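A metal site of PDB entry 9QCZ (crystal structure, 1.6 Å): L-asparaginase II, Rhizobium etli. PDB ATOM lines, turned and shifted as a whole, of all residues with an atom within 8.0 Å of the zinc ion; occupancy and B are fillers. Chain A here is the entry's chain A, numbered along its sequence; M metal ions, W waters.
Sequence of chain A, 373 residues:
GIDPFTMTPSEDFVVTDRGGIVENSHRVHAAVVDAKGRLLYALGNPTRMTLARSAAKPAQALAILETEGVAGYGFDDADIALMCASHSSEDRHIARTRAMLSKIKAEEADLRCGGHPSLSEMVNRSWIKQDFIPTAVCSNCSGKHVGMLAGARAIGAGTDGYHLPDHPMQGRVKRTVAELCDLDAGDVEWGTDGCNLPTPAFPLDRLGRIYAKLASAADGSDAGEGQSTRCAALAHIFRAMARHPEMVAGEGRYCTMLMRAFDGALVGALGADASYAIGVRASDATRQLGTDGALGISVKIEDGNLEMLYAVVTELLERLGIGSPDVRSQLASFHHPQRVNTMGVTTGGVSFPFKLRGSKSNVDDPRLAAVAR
The zinc ion is bound by NZ of Lys 144 (2.1 Å).
The zinc ion is bound by water W1.
SG of Cys 141 binds the zinc ion (2.3 Å).
The zinc ion is bound by SG of Cys 195 (2.3 Å).
The zinc ion has four donor atoms within binding distance.
Lys 57 touches the zinc ion.
Asp 193 touches the zinc ion (OD2 to ZN, 3.9 Å).
Of the 23 residues printed, 5 come within 4 Å of the zinc ion.
The side-chain hydroxyl of Thr 199 sits at hydrogen-bond distance from the side-chain carboxylate of Asp 193, 2.8 Å away.
The backbone carbonyl oxygen (O) of Ala 85 lies within hydrogen-bond range of the side-chain amino group (NZ) of Lys 57 (2.7 Å).
OG of Ser 139 sits at hydrogen-bond distance from N of Cys 141, at 2.9 Å.
SG of Cys 141 sits close to OD1 of Asn 140.
NZ of Lys 57 lies within hydrogen-bond range of OG of Ser 86, 2.9 Å away.
The side-chain amino group of Lys 57 lies within hydrogen-bond range of the side-chain amide oxygen of Asn 140 (3.0 Å).
The side-chain sulfur (SG) of Cys 141 sits close to the side-chain amino group (NZ) of Lys 57.
The backbone carbonyl oxygen (O) of Cys 195 lies within hydrogen-bond range of a ring nitrogen (NE2) of His 145 (3.1 Å).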
ATOM      1  N   ARG A  53     -29.528  -5.479 -24.680  1.00  0.00           N
ATOM      2  CA  ARG A  53     -28.365  -4.589 -24.816  1.00  0.00           C
ATOM      3  C   ARG A  53     -27.152  -5.344 -24.275  1.00  0.00           C
ATOM      4  O   ARG A  53     -26.968  -6.521 -24.609  1.00  0.00           O
ATOM      5  CB  ARG A  53     -28.659  -3.227 -24.161  1.00  0.00           C
ATOM      6  CG  ARG A  53     -29.948  -2.578 -24.665  1.00  0.00           C
ATOM      7  CD  ARG A  53     -29.832  -2.030 -26.078  1.00  0.00           C
ATOM      8  NE  ARG A  53     -28.763  -1.049 -26.137  1.00  0.00           N
ATOM      9  CZ  ARG A  53     -28.859   0.187 -25.623  1.00  0.00           C
ATOM     10  NH1 ARG A  53     -29.976   0.614 -25.044  1.00  0.00           N
ATOM     11  NH2 ARG A  53     -27.815   0.995 -25.708  1.00  0.00           N
ATOM     12  N   SER A  54     -26.325  -4.718 -23.441  1.00  0.00           N
ATOM     13  CA  SER A  54     -25.099  -5.343 -22.958  1.00  0.00           C
ATOM     14  C   SER A  54     -25.360  -6.520 -22.030  1.00  0.00           C
ATOM     15  O   SER A  54     -24.427  -7.258 -21.745  1.00  0.00           O
ATOM     16  CB  SER A  54     -24.206  -4.343 -22.231  1.00  0.00           C
ATOM     17  OG  SER A  54     -24.974  -3.559 -21.328  1.00  0.00           O
ATOM     18  N   LYS A  57     -24.235  -9.919 -23.318  1.00  0.00           N
ATOM     19  CA  LYS A  57     -22.829 -10.179 -23.601  1.00  0.00           C
ATOM     20  C   LYS A  57     -22.371 -11.583 -23.210  1.00  0.00           C
ATOM     21  O   LYS A  57     -21.512 -12.132 -23.934  1.00  0.00           O
ATOM     22  CB  LYS A  57     -21.929  -9.113 -22.942  1.00  0.00           C
ATOM     23  CG  LYS A  57     -21.902  -7.800 -23.727  1.00  0.00           C
ATOM     24  CD  LYS A  57     -21.211  -6.660 -22.929  1.00  0.00           C
ATOM     25  CE  LYS A  57     -21.128  -5.394 -23.838  1.00  0.00           C
ATOM     26  NZ  LYS A  57     -20.716  -4.149 -23.080  1.00  0.00           N
ATOM     27  N   GLN A  60     -23.097 -13.572 -26.278  1.00  0.00           N
ATOM     28  CA  GLN A  60     -22.149 -13.284 -27.346  1.00  0.00           C
ATOM     29  C   GLN A  60     -20.798 -13.884 -27.044  1.00  0.00           C
ATOM     30  O   GLN A  60     -20.111 -14.366 -27.958  1.00  0.00           O
ATOM     31  CB  GLN A  60     -22.055 -11.765 -27.556  1.00  0.00           C
ATOM     32  CG  GLN A  60     -23.401 -11.239 -28.101  1.00  0.00           C
ATOM     33  CD  GLN A  60     -23.603  -9.750 -27.835  1.00  0.00           C
ATOM     34  OE1 GLN A  60     -23.572  -9.296 -26.686  1.00  0.00           O
ATOM     35  NE2 GLN A  60     -23.785  -8.954 -28.932  1.00  0.00           N
ATOM     36  N   MET A  83     -14.640  -9.717 -22.389  1.00  0.00           N
ATOM     37  CA  MET A  83     -15.655  -9.951 -23.429  1.00  0.00           C
ATOM     38  C   MET A  83     -17.068  -9.800 -22.867  1.00  0.00           C
ATOM     39  O   MET A  83     -17.983  -9.359 -23.590  1.00  0.00           O
ATOM     40  CB  MET A  83     -15.486 -11.352 -24.061  1.00  0.00           C
ATOM     41  CG  MET A  83     -14.125 -11.607 -24.681  1.00  0.00           C
ATOM     42  SD  MET A  83     -14.145 -13.282 -25.365  1.00  0.00           S
ATOM     43  CE  MET A  83     -12.387 -13.497 -25.728  1.00  0.00           C
ATOM     44  N   ALA A  85     -17.958  -7.713 -20.558  1.00  0.00           N
ATOM     45  CA  ALA A  85     -17.939  -6.461 -19.801  1.00  0.00           C
ATOM     46  C   ALA A  85     -18.642  -5.279 -20.493  1.00  0.00           C
ATOM     47  O   ALA A  85     -18.661  -5.179 -21.719  1.00  0.00           O
ATOM     48  CB  ALA A  85     -16.504  -6.027 -19.560  1.00  0.00           C
ATOM     49  N   SER A  86     -19.210  -4.393 -19.667  1.00  0.00           N
ATOM     50  CA  SER A  86     -19.493  -2.996 -20.022  1.00  0.00           C
ATOM     51  C   SER A  86     -18.548  -2.189 -19.125  1.00  0.00           C
ATOM     52  O   SER A  86     -18.947  -1.654 -18.090  1.00  0.00           O
ATOM     53  CB  SER A  86     -20.991  -2.562 -19.790  1.00  0.00           C
ATOM     54  OG  SER A  86     -21.866  -3.393 -20.545  1.00  0.00           O
ATOM     55  N   CYS A 113     -16.222  -0.625 -33.374  1.00  0.00           N
ATOM     56  CA  CYS A 113     -16.868   0.140 -32.310  1.00  0.00           C
ATOM     57  C   CYS A 113     -16.175   1.490 -32.156  1.00  0.00           C
ATOM     58  O   CYS A 113     -15.017   1.682 -32.539  1.00  0.00           O
ATOM     59  CB  CYS A 113     -16.812  -0.608 -30.973  1.00  0.00           C
ATOM     60  SG  CYS A 113     -15.153  -1.181 -30.470  1.00  0.00           S
ATOM     61  N   SER A 139     -13.977   1.772 -25.985  1.00  0.00           N
ATOM     62  CA  SER A 139     -15.378   1.383 -25.900  1.00  0.00           C
ATOM     63  C   SER A 139     -15.602   0.411 -24.760  1.00  0.00           C
ATOM     64  O   SER A 139     -14.818  -0.533 -24.567  1.00  0.00           O
ATOM     65  CB  SER A 139     -15.817   0.697 -27.202  1.00  0.00           C
ATOM     66  OG  SER A 139     -17.026  -0.033 -27.060  1.00  0.00           O
ATOM     67  N   ASN A 140     -16.719   0.615 -24.030  1.00  0.00           N
ATOM     68  CA  ASN A 140     -17.107  -0.318 -22.969  1.00  0.00           C
ATOM     69  C   ASN A 140     -17.319  -1.723 -23.510  1.00  0.00           C
ATOM     70  O   ASN A 140     -17.229  -2.689 -22.735  1.00  0.00           O
ATOM     71  CB  ASN A 140     -18.391   0.188 -22.278  1.00  0.00           C
ATOM     72  CG  ASN A 140     -19.668  -0.195 -23.008  1.00  0.00           C
ATOM     73  OD1 ASN A 140     -20.336  -1.178 -22.633  1.00  0.00           O
ATOM     74  ND2 ASN A 140     -20.083   0.607 -23.989  1.00  0.00           N
ATOM     75  N   CYS A 141     -17.567  -1.848 -24.825  1.00  0.00           N
ATOM     76  CA  CYS A 141     -17.763  -3.124 -25.508  1.00  0.00           C
ATOM     77  C   CYS A 141     -16.488  -3.636 -26.178  1.00  0.00           C
ATOM     78  O   CYS A 141     -16.572  -4.597 -26.960  1.00  0.00           O
ATOM     79  CB  CYS A 141     -18.860  -2.999 -26.560  1.00  0.00           C
ATOM     80  SG  CYS A 141     -20.494  -2.538 -25.842  1.00  0.00           S
ATOM     81  N   SER A 142     -15.342  -3.028 -25.895  1.00  0.00           N
ATOM     82  CA  SER A 142     -14.124  -3.344 -26.650  1.00  0.00           C
ATOM     83  C   SER A 142     -13.734  -4.819 -26.559  1.00  0.00           C
ATOM     84  O   SER A 142     -13.240  -5.380 -27.555  1.00  0.00           O
ATOM     85  CB  SER A 142     -12.961  -2.449 -26.211  1.00  0.00           C
ATOM     86  OG  SER A 142     -12.636  -2.774 -24.874  1.00  0.00           O
ATOM     87  N   LYS A 144     -15.748  -7.550 -26.183  1.00  0.00           N
ATOM     88  CA  LYS A 144     -16.634  -8.288 -27.083  1.00  0.00           C
ATOM     89  C   LYS A 144     -16.178  -8.115 -28.539  1.00  0.00           C
ATOM     90  O   LYS A 144     -16.161  -9.084 -29.320  1.00  0.00           O
ATOM     91  CB  LYS A 144     -18.075  -7.779 -26.890  1.00  0.00           C
ATOM     92  CG  LYS A 144     -19.096  -8.257 -27.948  1.00  0.00           C
ATOM     93  CD  LYS A 144     -20.521  -7.736 -27.691  1.00  0.00           C
ATOM     94  CE  LYS A 144     -20.594  -6.189 -27.487  1.00  0.00           C
ATOM     95  NZ  LYS A 144     -22.030  -5.673 -27.513  1.00  0.00           N
ATOM     96  N   HIS A 145     -15.822  -6.874 -28.919  1.00  0.00           N
ATOM     97  CA  HIS A 145     -15.416  -6.664 -30.301  1.00  0.00           C
ATOM     98  C   HIS A 145     -14.115  -7.400 -30.641  1.00  0.00           C
ATOM     99  O   HIS A 145     -13.949  -7.914 -31.761  1.00  0.00           O
ATOM    100  CB  HIS A 145     -15.294  -5.153 -30.578  1.00  0.00           C
ATOM    101  CG  HIS A 145     -16.618  -4.516 -30.900  1.00  0.00           C
ATOM    102  ND1 HIS A 145     -16.981  -4.181 -32.183  1.00  0.00           N
ATOM    103  CD2 HIS A 145     -17.669  -4.187 -30.107  1.00  0.00           C
ATOM    104  CE1 HIS A 145     -18.196  -3.653 -32.171  1.00  0.00           C
ATOM    105  NE2 HIS A 145     -18.647  -3.664 -30.928  1.00  0.00           N
ATOM    106  N   MET A 148     -15.014 -10.934 -31.256  1.00  0.00           N
ATOM    107  CA  MET A 148     -15.625 -11.206 -32.552  1.00  0.00           C
ATOM    108  C   MET A 148     -14.613 -11.121 -33.684  1.00  0.00           C
ATOM    109  O   MET A 148     -14.724 -11.896 -34.649  1.00  0.00           O
ATOM    110  CB  MET A 148     -16.801 -10.278 -32.772  1.00  0.00           C
ATOM    111  CG  MET A 148     -17.919 -10.640 -31.849  1.00  0.00           C
ATOM    112  SD  MET A 148     -19.235  -9.460 -31.984  1.00  0.00           S
ATOM    113  CE  MET A 148     -20.476 -10.189 -30.936  1.00  0.00           C
ATOM    114  N   THR A 192     -29.476  -2.350 -33.636  1.00  0.00           N
ATOM    115  CA  THR A 192     -28.045  -2.067 -33.620  1.00  0.00           C
ATOM    116  C   THR A 192     -27.704  -1.324 -32.337  1.00  0.00           C
ATOM    117  O   THR A 192     -28.418  -0.391 -31.948  1.00  0.00           O
ATOM    118  CB  THR A 192     -27.632  -1.257 -34.869  1.00  0.00           C
ATOM    119  OG1 THR A 192     -27.928  -1.981 -36.075  1.00  0.00           O
ATOM    120  CG2 THR A 192     -26.136  -0.924 -34.828  1.00  0.00           C
ATOM    121  N   ASP A 193     -26.628  -1.732 -31.682  1.00  0.00           N
ATOM    122  CA  ASP A 193     -26.218  -1.239 -30.367  1.00  0.00           C
ATOM    123  C   ASP A 193     -25.373   0.028 -30.500  1.00  0.00           C
ATOM    124  O   ASP A 193     -24.967   0.423 -31.604  1.00  0.00           O
ATOM    125  CB  ASP A 193     -25.406  -2.327 -29.614  1.00  0.00           C
ATOM    126  CG  ASP A 193     -26.122  -2.873 -28.393  1.00  0.00           C
ATOM    127  OD1 ASP A 193     -27.058  -2.194 -27.907  1.00  0.00           O
ATOM    128  OD2 ASP A 193     -25.759  -4.002 -27.906  1.00  0.00           O
ATOM    129  N   GLY A 194     -25.084   0.674 -29.386  1.00  0.00           N
ATOM    130  CA  GLY A 194     -24.207   1.857 -29.426  1.00  0.00           C
ATOM    131  C   GLY A 194     -22.812   1.509 -29.918  1.00  0.00           C
ATOM    132  O   GLY A 194     -22.170   2.366 -30.521  1.00  0.00           O
ATOM    133  N   CYS A 195     -22.394   0.270 -29.694  1.00  0.00           N
ATOM    134  CA  CYS A 195     -21.050  -0.194 -30.140  1.00  0.00           C
ATOM    135  C   CYS A 195     -21.077  -0.659 -31.599  1.00  0.00           C
ATOM    136  O   CYS A 195     -20.073  -1.192 -32.030  1.00  0.00           O
ATOM    137  CB  CYS A 195     -20.546  -1.307 -29.252  1.00  0.00           C
ATOM    138  SG  CYS A 195     -21.517  -2.817 -29.464  1.00  0.00           S
ATOM    139  N   ASN A 196     -22.234  -0.579 -32.264  1.00  0.00           N
ATOM    140  CA  ASN A 196     -22.353  -0.822 -33.694  1.00  0.00           C
ATOM    141  C   ASN A 196     -22.441  -2.310 -34.038  1.00  0.00           C
ATOM    142  O   ASN A 196     -22.133  -2.698 -35.158  1.00  0.00           O
ATOM    143  CB  ASN A 196     -21.205  -0.156 -34.465  1.00  0.00           C
ATOM    144  CG  ASN A 196     -21.532   0.132 -35.908  1.00  0.00           C
ATOM    145  OD1 ASN A 196     -22.691   0.450 -36.251  1.00  0.00           O
ATOM    146  ND2 ASN A 196     -20.505   0.028 -36.801  1.00  0.00           N
ATOM    147  N   LEU A 197     -22.859  -3.160 -33.101  1.00  0.00           N
ATOM    148  CA  LEU A 197     -23.141  -4.578 -33.378  1.00  0.00           C
ATOM    149  C   LEU A 197     -24.631  -4.847 -33.389  1.00  0.00           C
ATOM    150  O   LEU A 197     -25.391  -4.110 -32.749  1.00  0.00           O
ATOM    151  CB  LEU A 197     -22.521  -5.462 -32.294  1.00  0.00           C
ATOM    152  CG  LEU A 197     -21.026  -5.768 -32.423  1.00  0.00           C
ATOM    153  CD1 LEU A 197     -20.501  -6.315 -31.105  1.00  0.00           C
ATOM    154  CD2 LEU A 197     -20.757  -6.764 -33.613  1.00  0.00           C
ATOM    155  N   PRO A 198     -25.092  -5.931 -34.033  1.00  0.00           N
ATOM    156  CA  PRO A 198     -26.490  -6.359 -33.857  1.00  0.00           C
ATOM    157  C   PRO A 198     -26.753  -6.637 -32.390  1.00  0.00           C
ATOM    158  O   PRO A 198     -25.882  -7.130 -31.666  1.00  0.00           O
ATOM    159  CB  PRO A 198     -26.573  -7.662 -34.672  1.00  0.00           C
ATOM    160  CG  PRO A 198     -25.446  -7.496 -35.725  1.00  0.00           C
ATOM    161  CD  PRO A 198     -24.356  -6.876 -34.903  1.00  0.00           C
ATOM    162  N   THR A 199     -27.950  -6.268 -31.923  1.00  0.00           N
ATOM    163  CA  THR A 199     -28.292  -6.478 -30.518  1.00  0.00           C
ATOM    164  C   THR A 199     -29.711  -7.038 -30.383  1.00  0.00           C
ATOM    165  O   THR A 199     -30.610  -6.631 -31.144  1.00  0.00           O
ATOM    166  CB  THR A 199     -28.125  -5.140 -29.754  1.00  0.00           C
ATOM    167  OG1 THR A 199     -28.185  -5.402 -28.352  1.00  0.00           O
ATOM    168  CG2 THR A 199     -29.156  -4.053 -30.136  1.00  0.00           C
HETATM  169 ZN    ZN M   1     -21.938  -3.581 -27.310  1.00  0.00          ZN
HETATM  170  O   HOH W   1     -23.751  -3.399 -26.228  1.00  0.00           O
